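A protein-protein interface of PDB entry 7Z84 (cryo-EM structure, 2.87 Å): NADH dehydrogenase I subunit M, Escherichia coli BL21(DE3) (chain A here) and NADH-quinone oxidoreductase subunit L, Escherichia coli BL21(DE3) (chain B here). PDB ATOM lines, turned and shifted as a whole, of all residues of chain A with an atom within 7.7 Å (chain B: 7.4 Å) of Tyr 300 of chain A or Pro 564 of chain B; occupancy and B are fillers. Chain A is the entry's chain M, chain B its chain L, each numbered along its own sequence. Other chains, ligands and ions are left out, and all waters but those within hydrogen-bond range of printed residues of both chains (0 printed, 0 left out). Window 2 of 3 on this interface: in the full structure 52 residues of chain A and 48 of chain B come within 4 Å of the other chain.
The backbone nitrogen of Pro 564 of chain B sits close to the side-chain hydroxyl of Tyr 300 of chain A (3.3 Å).
SD of Met 304 of chain A sits close to O of Leu 560 of chain B, at 3.1 Å.
The backbone NH of Leu 565 of chain B sits at hydrogen-bond distance from the side-chain hydroxyl of Tyr 300 of chain A.
The side-chain carboxylate of Asp 563 of chain B sits at hydrogen-bond distance from the side-chain hydroxyl of Tyr 317 of chain A (2.7 Å).
The side-chain carboxylate of Asp 563 of chain B sits at hydrogen-bond distance from a ring nitrogen (NE2) of His 241 of chain A (3.1 Å).
The side-chain hydroxyl (OH) of Tyr 300 of chain A is in hydrogen-bond range of the side-chain carboxylate (OD1) of Asp 563 of chain B, 2.5 Å away.
Among the printed residues, merely in contact across the chains: His 241 of chain A with Leu 565 of chain B, Pro 239 of chain A with Met 569 of chain B, Pro 239 of chain A with Leu 565 of chain B, Gly 242 of chain A with Asn 566 of chain B and Met 304 of chain A with Asp 563 of chain B.
O of Pro 239 of chain A lies close to ND1 of His 241 of chain A (3.4 Å).
Of chain B, only Asp 563, Pro 564 and Leu 565 come within 4 Å of Tyr 300 of chain A.
Of the printed residues of chain A, Asp 563 of chain B touches His 241 (3.1 Å), Tyr 300 (2.5 Å), Met 304 (3.8 Å) and Tyr 317 (2.7 Å).
Printed residues of chain A within 4 Å of Asn 566 of chain B: Gly 242.
The nearest printed residue of chain A that does not touch Asp 563 of chain B is Gly 242 of chain A (4.7 Å).
Of the 23 printed residues of chain A, 6 touch a printed residue of chain B.
Of the 13 printed residues of chain B, 6 touch a printed residue of chain A.
Among the printed residues, 11 pairs touch across the chains.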
ATOM      1  N   VAL A 238     -16.808   9.617  15.061  1.00  0.00           N
ATOM      2  CA  VAL A 238     -15.720   9.403  14.096  1.00  0.00           C
ATOM      3  C   VAL A 238     -16.113   9.986  12.743  1.00  0.00           C
ATOM      4  O   VAL A 238     -17.299   9.919  12.360  1.00  0.00           O
ATOM      5  CB  VAL A 238     -15.390   7.905  13.978  1.00  0.00           C
ATOM      6  CG1 VAL A 238     -14.624   7.434  15.203  1.00  0.00           C
ATOM      7  CG2 VAL A 238     -16.657   7.088  13.795  1.00  0.00           C
ATOM      8  N   PRO A 239     -15.183  10.585  11.981  1.00  0.00           N
ATOM      9  CA  PRO A 239     -13.754  10.753  12.273  1.00  0.00           C
ATOM     10  C   PRO A 239     -13.415  12.052  13.004  1.00  0.00           C
ATOM     11  O   PRO A 239     -12.257  12.468  13.011  1.00  0.00           O
ATOM     12  CB  PRO A 239     -13.129  10.747  10.884  1.00  0.00           C
ATOM     13  CG  PRO A 239     -14.168  11.379  10.020  1.00  0.00           C
ATOM     14  CD  PRO A 239     -15.518  11.092  10.640  1.00  0.00           C
ATOM     15  N   HIS A 241     -12.859  12.952  16.002  1.00  0.00           N
ATOM     16  CA  HIS A 241     -12.603  12.444  17.345  1.00  0.00           C
ATOM     17  C   HIS A 241     -11.197  12.671  17.880  1.00  0.00           C
ATOM     18  O   HIS A 241     -11.038  12.678  19.105  1.00  0.00           O
ATOM     19  CB  HIS A 241     -12.895  10.938  17.407  1.00  0.00           C
ATOM     20  CG  HIS A 241     -11.977  10.117  16.560  1.00  0.00           C
ATOM     21  ND1 HIS A 241     -12.206   9.888  15.221  1.00  0.00           N
ATOM     22  CD2 HIS A 241     -10.818   9.484  16.857  1.00  0.00           C
ATOM     23  CE1 HIS A 241     -11.232   9.142  14.732  1.00  0.00           C
ATOM     24  NE2 HIS A 241     -10.376   8.885  15.704  1.00  0.00           N
ATOM     25  N   GLY A 242     -10.182  12.863  17.029  1.00  0.00           N
ATOM     26  CA  GLY A 242      -8.794  12.883  17.482  1.00  0.00           C
ATOM     27  C   GLY A 242      -8.452  14.028  18.414  1.00  0.00           C
ATOM     28  O   GLY A 242      -7.481  13.930  19.185  1.00  0.00           O
ATOM     29  N   LEU A 293     -22.553   5.225  12.006  1.00  0.00           N
ATOM     30  CA  LEU A 293     -21.438   6.003  12.536  1.00  0.00           C
ATOM     31  C   LEU A 293     -21.202   5.684  14.005  1.00  0.00           C
ATOM     32  O   LEU A 293     -20.057   5.642  14.459  1.00  0.00           O
ATOM     33  CB  LEU A 293     -21.702   7.496  12.354  1.00  0.00           C
ATOM     34  CG  LEU A 293     -21.377   8.108  10.992  1.00  0.00           C
ATOM     35  CD1 LEU A 293     -21.898   9.530  10.929  1.00  0.00           C
ATOM     36  CD2 LEU A 293     -19.884   8.066  10.721  1.00  0.00           C
ATOM     37  N   GLY A 294     -22.277   5.454  14.761  1.00  0.00           N
ATOM     38  CA  GLY A 294     -22.126   5.048  16.151  1.00  0.00           C
ATOM     39  C   GLY A 294     -21.493   3.676  16.304  1.00  0.00           C
ATOM     40  O   GLY A 294     -20.669   3.462  17.198  1.00  0.00           O
ATOM     41  N   VAL A 295     -21.876   2.728  15.442  1.00  0.00           N
ATOM     42  CA  VAL A 295     -21.270   1.393  15.454  1.00  0.00           C
ATOM     43  C   VAL A 295     -19.779   1.480  15.132  1.00  0.00           C
ATOM     44  O   VAL A 295     -18.930   0.880  15.818  1.00  0.00           O
ATOM     45  CB  VAL A 295     -22.005   0.469  14.464  1.00  0.00           C
ATOM     46  CG1 VAL A 295     -21.134  -0.711  14.058  1.00  0.00           C
ATOM     47  CG2 VAL A 295     -23.309  -0.024  15.054  1.00  0.00           C
ATOM     48  N   ILE A 296     -19.444   2.241  14.084  1.00  0.00           N
ATOM     49  CA  ILE A 296     -18.049   2.436  13.694  1.00  0.00           C
ATOM     50  C   ILE A 296     -17.282   3.140  14.805  1.00  0.00           C
ATOM     51  O   ILE A 296     -16.128   2.807  15.083  1.00  0.00           O
ATOM     52  CB  ILE A 296     -17.975   3.202  12.358  1.00  0.00           C
ATOM     53  CG1 ILE A 296     -18.468   2.321  11.209  1.00  0.00           C
ATOM     54  CG2 ILE A 296     -16.562   3.681  12.058  1.00  0.00           C
ATOM     55  CD1 ILE A 296     -18.636   3.065   9.904  1.00  0.00           C
ATOM     56  N   GLY A 297     -17.926   4.090  15.486  1.00  0.00           N
ATOM     57  CA  GLY A 297     -17.287   4.760  16.604  1.00  0.00           C
ATOM     58  C   GLY A 297     -17.008   3.833  17.769  1.00  0.00           C
ATOM     59  O   GLY A 297     -15.939   3.902  18.375  1.00  0.00           O
ATOM     60  N   ILE A 298     -17.954   2.938  18.079  1.00  0.00           N
ATOM     61  CA  ILE A 298     -17.761   1.970  19.160  1.00  0.00           C
ATOM     62  C   ILE A 298     -16.566   1.074  18.864  1.00  0.00           C
ATOM     63  O   ILE A 298     -15.644   0.944  19.683  1.00  0.00           O
ATOM     64  CB  ILE A 298     -19.034   1.132  19.372  1.00  0.00           C
ATOM     65  CG1 ILE A 298     -20.117   1.942  20.072  1.00  0.00           C
ATOM     66  CG2 ILE A 298     -18.732  -0.124  20.179  1.00  0.00           C
ATOM     67  CD1 ILE A 298     -21.425   1.213  20.162  1.00  0.00           C
ATOM     68  N   PHE A 299     -16.539   0.484  17.668  1.00  0.00           N
ATOM     69  CA  PHE A 299     -15.467  -0.465  17.373  1.00  0.00           C
ATOM     70  C   PHE A 299     -14.131   0.227  17.141  1.00  0.00           C
ATOM     71  O   PHE A 299     -13.085  -0.294  17.550  1.00  0.00           O
ATOM     72  CB  PHE A 299     -15.854  -1.337  16.187  1.00  0.00           C
ATOM     73  CG  PHE A 299     -16.705  -2.493  16.575  1.00  0.00           C
ATOM     74  CD1 PHE A 299     -16.127  -3.686  16.974  1.00  0.00           C
ATOM     75  CD2 PHE A 299     -18.077  -2.368  16.622  1.00  0.00           C
ATOM     76  CE1 PHE A 299     -16.908  -4.751  17.361  1.00  0.00           C
ATOM     77  CE2 PHE A 299     -18.855  -3.421  17.015  1.00  0.00           C
ATOM     78  CZ  PHE A 299     -18.275  -4.618  17.381  1.00  0.00           C
ATOM     79  N   TYR A 300     -14.145   1.403  16.513  1.00  0.00           N
ATOM     80  CA  TYR A 300     -12.925   2.171  16.327  1.00  0.00           C
ATOM     81  C   TYR A 300     -12.344   2.606  17.664  1.00  0.00           C
ATOM     82  O   TYR A 300     -11.138   2.473  17.885  1.00  0.00           O
ATOM     83  CB  TYR A 300     -13.213   3.380  15.440  1.00  0.00           C
ATOM     84  CG  TYR A 300     -11.984   4.048  14.878  1.00  0.00           C
ATOM     85  CD1 TYR A 300     -11.422   3.617  13.684  1.00  0.00           C
ATOM     86  CD2 TYR A 300     -11.392   5.117  15.533  1.00  0.00           C
ATOM     87  CE1 TYR A 300     -10.299   4.226  13.165  1.00  0.00           C
ATOM     88  CE2 TYR A 300     -10.270   5.731  15.023  1.00  0.00           C
ATOM     89  CZ  TYR A 300      -9.730   5.284  13.839  1.00  0.00           C
ATOM     90  OH  TYR A 300      -8.612   5.901  13.331  1.00  0.00           O
ATOM     91  N   GLY A 301     -13.185   3.101  18.575  1.00  0.00           N
ATOM     92  CA  GLY A 301     -12.698   3.496  19.884  1.00  0.00           C
ATOM     93  C   GLY A 301     -12.185   2.320  20.691  1.00  0.00           C
ATOM     94  O   GLY A 301     -11.201   2.447  21.421  1.00  0.00           O
ATOM     95  N   ALA A 302     -12.828   1.156  20.553  1.00  0.00           N
ATOM     96  CA  ALA A 302     -12.333  -0.038  21.230  1.00  0.00           C
ATOM     97  C   ALA A 302     -10.967  -0.461  20.698  1.00  0.00           C
ATOM     98  O   ALA A 302     -10.061  -0.783  21.482  1.00  0.00           O
ATOM     99  CB  ALA A 302     -13.341  -1.176  21.083  1.00  0.00           C
ATOM    100  N   TRP A 303     -10.792  -0.449  19.373  1.00  0.00           N
ATOM    101  CA  TRP A 303      -9.515  -0.859  18.797  1.00  0.00           C
ATOM    102  C   TRP A 303      -8.411   0.150  19.096  1.00  0.00           C
ATOM    103  O   TRP A 303      -7.251  -0.236  19.283  1.00  0.00           O
ATOM    104  CB  TRP A 303      -9.651  -1.076  17.291  1.00  0.00           C
ATOM    105  CG  TRP A 303      -9.893  -2.507  16.914  1.00  0.00           C
ATOM    106  CD1 TRP A 303      -9.126  -3.580  17.254  1.00  0.00           C
ATOM    107  CD2 TRP A 303     -10.954  -3.016  16.096  1.00  0.00           C
ATOM    108  NE1 TRP A 303      -9.652  -4.728  16.717  1.00  0.00           N
ATOM    109  CE2 TRP A 303     -10.775  -4.410  16.001  1.00  0.00           C
ATOM    110  CE3 TRP A 303     -12.041  -2.431  15.442  1.00  0.00           C
ATOM    111  CZ2 TRP A 303     -11.637  -5.225  15.273  1.00  0.00           C
ATOM    112  CZ3 TRP A 303     -12.901  -3.242  14.726  1.00  0.00           C
ATOM    113  CH2 TRP A 303     -12.695  -4.625  14.648  1.00  0.00           C
ATOM    114  N   MET A 304      -8.742   1.444  19.130  1.00  0.00           N
ATOM    115  CA  MET A 304      -7.762   2.439  19.555  1.00  0.00           C
ATOM    116  C   MET A 304      -7.399   2.273  21.025  1.00  0.00           C
ATOM    117  O   MET A 304      -6.221   2.359  21.386  1.00  0.00           O
ATOM    118  CB  MET A 304      -8.274   3.859  19.300  1.00  0.00           C
ATOM    119  CG  MET A 304      -8.573   4.246  17.861  1.00  0.00           C
ATOM    120  SD  MET A 304      -7.163   4.408  16.762  1.00  0.00           S
ATOM    121  CE  MET A 304      -5.920   5.112  17.843  1.00  0.00           C
ATOM    122  N   ALA A 305      -8.395   2.030  21.887  1.00  0.00           N
ATOM    123  CA  ALA A 305      -8.142   1.920  23.320  1.00  0.00           C
ATOM    124  C   ALA A 305      -7.302   0.695  23.645  1.00  0.00           C
ATOM    125  O   ALA A 305      -6.477   0.730  24.564  1.00  0.00           O
ATOM    126  CB  ALA A 305      -9.462   1.877  24.085  1.00  0.00           C
ATOM    127  N   PHE A 306      -7.501  -0.402  22.911  1.00  0.00           N
ATOM    128  CA  PHE A 306      -6.656  -1.571  23.130  1.00  0.00           C
ATOM    129  C   PHE A 306      -5.214  -1.313  22.702  1.00  0.00           C
ATOM    130  O   PHE A 306      -4.283  -1.860  23.304  1.00  0.00           O
ATOM    131  CB  PHE A 306      -7.222  -2.781  22.391  1.00  0.00           C
ATOM    132  CG  PHE A 306      -6.386  -4.016  22.537  1.00  0.00           C
ATOM    133  CD1 PHE A 306      -6.334  -4.692  23.746  1.00  0.00           C
ATOM    134  CD2 PHE A 306      -5.642  -4.496  21.473  1.00  0.00           C
ATOM    135  CE1 PHE A 306      -5.562  -5.827  23.887  1.00  0.00           C
ATOM    136  CE2 PHE A 306      -4.868  -5.628  21.609  1.00  0.00           C
ATOM    137  CZ  PHE A 306      -4.829  -6.296  22.817  1.00  0.00           C
ATOM    138  N   TYR A 317     -10.494   7.034  24.467  1.00  0.00           N
ATOM    139  CA  TYR A 317     -11.124   6.160  23.482  1.00  0.00           C
ATOM    140  C   TYR A 317     -12.260   5.335  24.090  1.00  0.00           C
ATOM    141  O   TYR A 317     -13.207   4.971  23.375  1.00  0.00           O
ATOM    142  CB  TYR A 317     -10.068   5.277  22.826  1.00  0.00           C
ATOM    143  CG  TYR A 317      -9.189   6.043  21.863  1.00  0.00           C
ATOM    144  CD1 TYR A 317      -9.746   6.780  20.825  1.00  0.00           C
ATOM    145  CD2 TYR A 317      -7.807   6.035  21.989  1.00  0.00           C
ATOM    146  CE1 TYR A 317      -8.951   7.483  19.942  1.00  0.00           C
ATOM    147  CE2 TYR A 317      -7.004   6.735  21.112  1.00  0.00           C
ATOM    148  CZ  TYR A 317      -7.580   7.457  20.090  1.00  0.00           C
ATOM    149  OH  TYR A 317      -6.782   8.154  19.214  1.00  0.00           O
ATOM    150  N   VAL A 320     -14.980   7.629  23.603  1.00  0.00           N
ATOM    151  CA  VAL A 320     -15.422   7.567  22.207  1.00  0.00           C
ATOM    152  C   VAL A 320     -16.378   6.395  21.991  1.00  0.00           C
ATOM    153  O   VAL A 320     -17.429   6.539  21.350  1.00  0.00           O
ATOM    154  CB  VAL A 320     -14.204   7.487  21.265  1.00  0.00           C
ATOM    155  CG1 VAL A 320     -14.642   7.232  19.832  1.00  0.00           C
ATOM    156  CG2 VAL A 320     -13.389   8.765  21.342  1.00  0.00           C
ATOM    157  N   SER A 321     -16.041   5.223  22.542  1.00  0.00           N
ATOM    158  CA  SER A 321     -16.902   4.048  22.387  1.00  0.00           C
ATOM    159  C   SER A 321     -18.252   4.227  23.084  1.00  0.00           C
ATOM    160  O   SER A 321     -19.308   3.904  22.514  1.00  0.00           O
ATOM    161  CB  SER A 321     -16.185   2.809  22.922  1.00  0.00           C
ATOM    162  OG  SER A 321     -17.062   1.698  22.977  1.00  0.00           O
ATOM    163  N   PHE A 431     -15.773  -6.101  23.189  1.00  0.00           N
ATOM    164  CA  PHE A 431     -14.536  -5.363  22.916  1.00  0.00           C
ATOM    165  C   PHE A 431     -14.183  -4.416  24.064  1.00  0.00           C
ATOM    166  O   PHE A 431     -13.001  -4.218  24.386  1.00  0.00           O
ATOM    167  CB  PHE A 431     -14.682  -4.578  21.611  1.00  0.00           C
ATOM    168  CG  PHE A 431     -14.413  -5.382  20.366  1.00  0.00           C
ATOM    169  CD1 PHE A 431     -14.919  -6.664  20.211  1.00  0.00           C
ATOM    170  CD2 PHE A 431     -13.680  -4.833  19.329  1.00  0.00           C
ATOM    171  CE1 PHE A 431     -14.680  -7.388  19.063  1.00  0.00           C
ATOM    172  CE2 PHE A 431     -13.442  -5.552  18.178  1.00  0.00           C
ATOM    173  CZ  PHE A 431     -13.940  -6.832  18.046  1.00  0.00           C
ATOM    174  N   TYR A 435     -10.660  -4.284  26.241  1.00  0.00           N
ATOM    175  CA  TYR A 435      -9.719  -3.187  26.487  1.00  0.00           C
ATOM    176  C   TYR A 435      -9.615  -2.844  27.971  1.00  0.00           C
ATOM    177  O   TYR A 435      -8.543  -2.423  28.427  1.00  0.00           O
ATOM    178  CB  TYR A 435     -10.031  -1.940  25.628  1.00  0.00           C
ATOM    179  CG  TYR A 435     -11.340  -1.159  25.786  1.00  0.00           C
ATOM    180  CD1 TYR A 435     -11.756  -0.636  27.006  1.00  0.00           C
ATOM    181  CD2 TYR A 435     -12.100  -0.848  24.668  1.00  0.00           C
ATOM    182  CE1 TYR A 435     -12.929   0.077  27.120  1.00  0.00           C
ATOM    183  CE2 TYR A 435     -13.260  -0.102  24.766  1.00  0.00           C
ATOM    184  CZ  TYR A 435     -13.672   0.354  25.997  1.00  0.00           C
ATOM    185  OH  TYR A 435     -14.833   1.083  26.108  1.00  0.00           O
ATOM    186  N   LEU B 559      -2.561  -2.269  13.105  1.00  0.00           N
ATOM    187  CA  LEU B 559      -2.753  -1.427  11.929  1.00  0.00           C
ATOM    188  C   LEU B 559      -3.368  -0.080  12.301  1.00  0.00           C
ATOM    189  O   LEU B 559      -2.977   0.959  11.758  1.00  0.00           O
ATOM    190  CB  LEU B 559      -3.621  -2.160  10.905  1.00  0.00           C
ATOM    191  CG  LEU B 559      -4.449  -1.333   9.922  1.00  0.00           C
ATOM    192  CD1 LEU B 559      -3.587  -0.861   8.763  1.00  0.00           C
ATOM    193  CD2 LEU B 559      -5.637  -2.135   9.416  1.00  0.00           C
ATOM    194  N   LEU B 560      -4.316  -0.076  13.235  1.00  0.00           N
ATOM    195  CA  LEU B 560      -5.053   1.127  13.593  1.00  0.00           C
ATOM    196  C   LEU B 560      -4.415   1.921  14.724  1.00  0.00           C
ATOM    197  O   LEU B 560      -4.947   2.971  15.086  1.00  0.00           O
ATOM    198  CB  LEU B 560      -6.491   0.768  13.985  1.00  0.00           C
ATOM    199  CG  LEU B 560      -7.419   0.238  12.893  1.00  0.00           C
ATOM    200  CD1 LEU B 560      -8.816   0.022  13.450  1.00  0.00           C
ATOM    201  CD2 LEU B 560      -7.454   1.184  11.707  1.00  0.00           C
ATOM    202  N   LYS B 561      -3.291   1.458  15.283  1.00  0.00           N
ATOM    203  CA  LYS B 561      -2.665   2.161  16.403  1.00  0.00           C
ATOM    204  C   LYS B 561      -2.170   3.563  16.049  1.00  0.00           C
ATOM    205  O   LYS B 561      -1.890   4.350  16.958  1.00  0.00           O
ATOM    206  CB  LYS B 561      -1.499   1.336  16.951  1.00  0.00           C
ATOM    207  CG  LYS B 561      -0.246   1.385  16.095  1.00  0.00           C
ATOM    208  CD  LYS B 561       0.833   0.458  16.632  1.00  0.00           C
ATOM    209  CE  LYS B 561       1.985   0.319  15.648  1.00  0.00           C
ATOM    210  NZ  LYS B 561       1.592   0.692  14.260  1.00  0.00           N
ATOM    211  N   ARG B 562      -2.055   3.896  14.764  1.00  0.00           N
ATOM    212  CA  ARG B 562      -1.618   5.220  14.343  1.00  0.00           C
ATOM    213  C   ARG B 562      -2.777   6.155  14.013  1.00  0.00           C
ATOM    214  O   ARG B 562      -2.535   7.270  13.538  1.00  0.00           O
ATOM    215  CB  ARG B 562      -0.676   5.106  13.144  1.00  0.00           C
ATOM    216  CG  ARG B 562       0.788   4.936  13.526  1.00  0.00           C
ATOM    217  CD  ARG B 562       1.323   6.166  14.250  1.00  0.00           C
ATOM    218  NE  ARG B 562       1.379   5.986  15.697  1.00  0.00           N
ATOM    219  CZ  ARG B 562       2.335   5.327  16.339  1.00  0.00           C
ATOM    220  NH1 ARG B 562       3.348   4.773  15.693  1.00  0.00           N
ATOM    221  NH2 ARG B 562       2.275   5.227  17.663  1.00  0.00           N
ATOM    222  N   ASP B 563      -4.027   5.723  14.253  1.00  0.00           N
ATOM    223  CA  ASP B 563      -5.255   6.504  14.091  1.00  0.00           C
ATOM    224  C   ASP B 563      -5.416   7.033  12.667  1.00  0.00           C
ATOM    225  O   ASP B 563      -5.203   8.231  12.433  1.00  0.00           O
ATOM    226  CB  ASP B 563      -5.294   7.659  15.095  1.00  0.00           C
ATOM    227  CG  ASP B 563      -6.705   8.027  15.508  1.00  0.00           C
ATOM    228  OD1 ASP B 563      -7.656   7.644  14.795  1.00  0.00           O
ATOM    229  OD2 ASP B 563      -6.864   8.699  16.548  1.00  0.00           O
ATOM    230  N   PRO B 564      -5.744   6.174  11.693  1.00  0.00           N
ATOM    231  CA  PRO B 564      -5.844   6.638  10.295  1.00  0.00           C
ATOM    232  C   PRO B 564      -6.897   7.712  10.049  1.00  0.00           C
ATOM    233  O   PRO B 564      -6.699   8.558   9.170  1.00  0.00           O
ATOM    234  CB  PRO B 564      -6.175   5.352   9.524  1.00  0.00           C
ATOM    235  CG  PRO B 564      -5.737   4.241  10.415  1.00  0.00           C
ATOM    236  CD  PRO B 564      -5.979   4.725  11.805  1.00  0.00           C
ATOM    237  N   LEU B 565      -8.011   7.701  10.787  1.00  0.00           N
ATOM    238  CA  LEU B 565      -9.028   8.733  10.592  1.00  0.00           C
ATOM    239  C   LEU B 565      -8.544  10.097  11.068  1.00  0.00           C
ATOM    240  O   LEU B 565      -8.938  11.128  10.506  1.00  0.00           O
ATOM    241  CB  LEU B 565     -10.319   8.345  11.314  1.00  0.00           C
ATOM    242  CG  LEU B 565     -10.988   7.034  10.893  1.00  0.00           C
ATOM    243  CD1 LEU B 565     -12.362   6.909  11.529  1.00  0.00           C
ATOM    244  CD2 LEU B 565     -11.087   6.928   9.379  1.00  0.00           C
ATOM    245  N   ASN B 566      -7.683  10.119  12.089  1.00  0.00           N
ATOM    246  CA  ASN B 566      -7.076  11.370  12.529  1.00  0.00           C
ATOM    247  C   ASN B 566      -6.203  11.973  11.435  1.00  0.00           C
ATOM    248  O   ASN B 566      -6.250  13.183  11.192  1.00  0.00           O
ATOM    249  CB  ASN B 566      -6.261  11.135  13.800  1.00  0.00           C
ATOM    250  CG  ASN B 566      -6.064  12.397  14.605  1.00  0.00           C
ATOM    251  OD1 ASN B 566      -6.724  13.408  14.366  1.00  0.00           O
ATOM    252  ND2 ASN B 566      -5.154  12.349  15.569  1.00  0.00           N
ATOM    253  N   SER B 567      -5.418  11.141  10.746  1.00  0.00           N
ATOM    254  CA  SER B 567      -4.628  11.627   9.617  1.00  0.00           C
ATOM    255  C   SER B 567      -5.521  12.032   8.449  1.00  0.00           C
ATOM    256  O   SER B 567      -5.213  12.990   7.726  1.00  0.00           O
ATOM    257  CB  SER B 567      -3.627  10.558   9.184  1.00  0.00           C
ATOM    258  OG  SER B 567      -2.891  10.074  10.293  1.00  0.00           O
ATOM    259  N   MET B 568      -6.631  11.314   8.256  1.00  0.00           N
ATOM    260  CA  MET B 568      -7.567  11.645   7.187  1.00  0.00           C
ATOM    261  C   MET B 568      -8.173  13.027   7.391  1.00  0.00           C
ATOM    262  O   MET B 568      -8.316  13.798   6.434  1.00  0.00           O
ATOM    263  CB  MET B 568      -8.664  10.580   7.111  1.00  0.00           C
ATOM    264  CG  MET B 568      -9.777  10.885   6.123  1.00  0.00           C
ATOM    265  SD  MET B 568     -11.396  10.387   6.742  1.00  0.00           S
ATOM    266  CE  MET B 568     -12.242  10.010   5.211  1.00  0.00           C
ATOM    267  N   MET B 569      -8.526  13.365   8.629  1.00  0.00           N
ATOM    268  CA  MET B 569      -9.028  14.708   8.895  1.00  0.00           C
ATOM    269  C   MET B 569      -7.923  15.733   9.127  1.00  0.00           C
ATOM    270  O   MET B 569      -8.218  16.933   9.164  1.00  0.00           O
ATOM    271  CB  MET B 569      -9.987  14.702  10.083  1.00  0.00           C
ATOM    272  CG  MET B 569     -11.269  13.948   9.811  1.00  0.00           C
ATOM    273  SD  MET B 569     -12.105  14.614   8.358  1.00  0.00           S
ATOM    274  CE  MET B 569     -12.864  16.088   9.023  1.00  0.00           C
ATOM    275  N   ASN B 570      -6.673  15.302   9.300  1.00  0.00           N
ATOM    276  CA  ASN B 570      -5.550  16.231   9.331  1.00  0.00           C
ATOM    277  C   ASN B 570      -5.012  16.550   7.944  1.00  0.00           C
ATOM    278  O   ASN B 570      -4.164  17.438   7.818  1.00  0.00           O
ATOM    279  CB  ASN B 570      -4.421  15.667  10.198  1.00  0.00           C
ATOM    280  CG  ASN B 570      -4.616  15.955  11.671  1.00  0.00           C
ATOM    281  OD1 ASN B 570      -5.568  16.628  12.065  1.00  0.00           O
ATOM    282  ND2 ASN B 570      -3.711  15.445  12.497  1.00  0.00           N
ATOM    283  N   ILE B 571      -5.452  15.818   6.925  1.00  0.00           N
ATOM    284  CA  ILE B 571      -5.138  16.111   5.523  1.00  0.00           C
ATOM    285  C   ILE B 571      -5.520  17.543   5.122  1.00  0.00           C
ATOM    286  O   ILE B 571      -4.711  18.196   4.438  1.00  0.00           O
ATOM    287  CB  ILE B 571      -5.776  15.050   4.600  1.00  0.00           C
ATOM    288  CG1 ILE B 571      -4.857  13.833   4.472  1.00  0.00           C
ATOM    289  CG2 ILE B 571      -6.117  15.608   3.219  1.00  0.00           C
ATOM    290  CD1 ILE B 571      -5.488  12.669   3.742  1.00  0.00           C
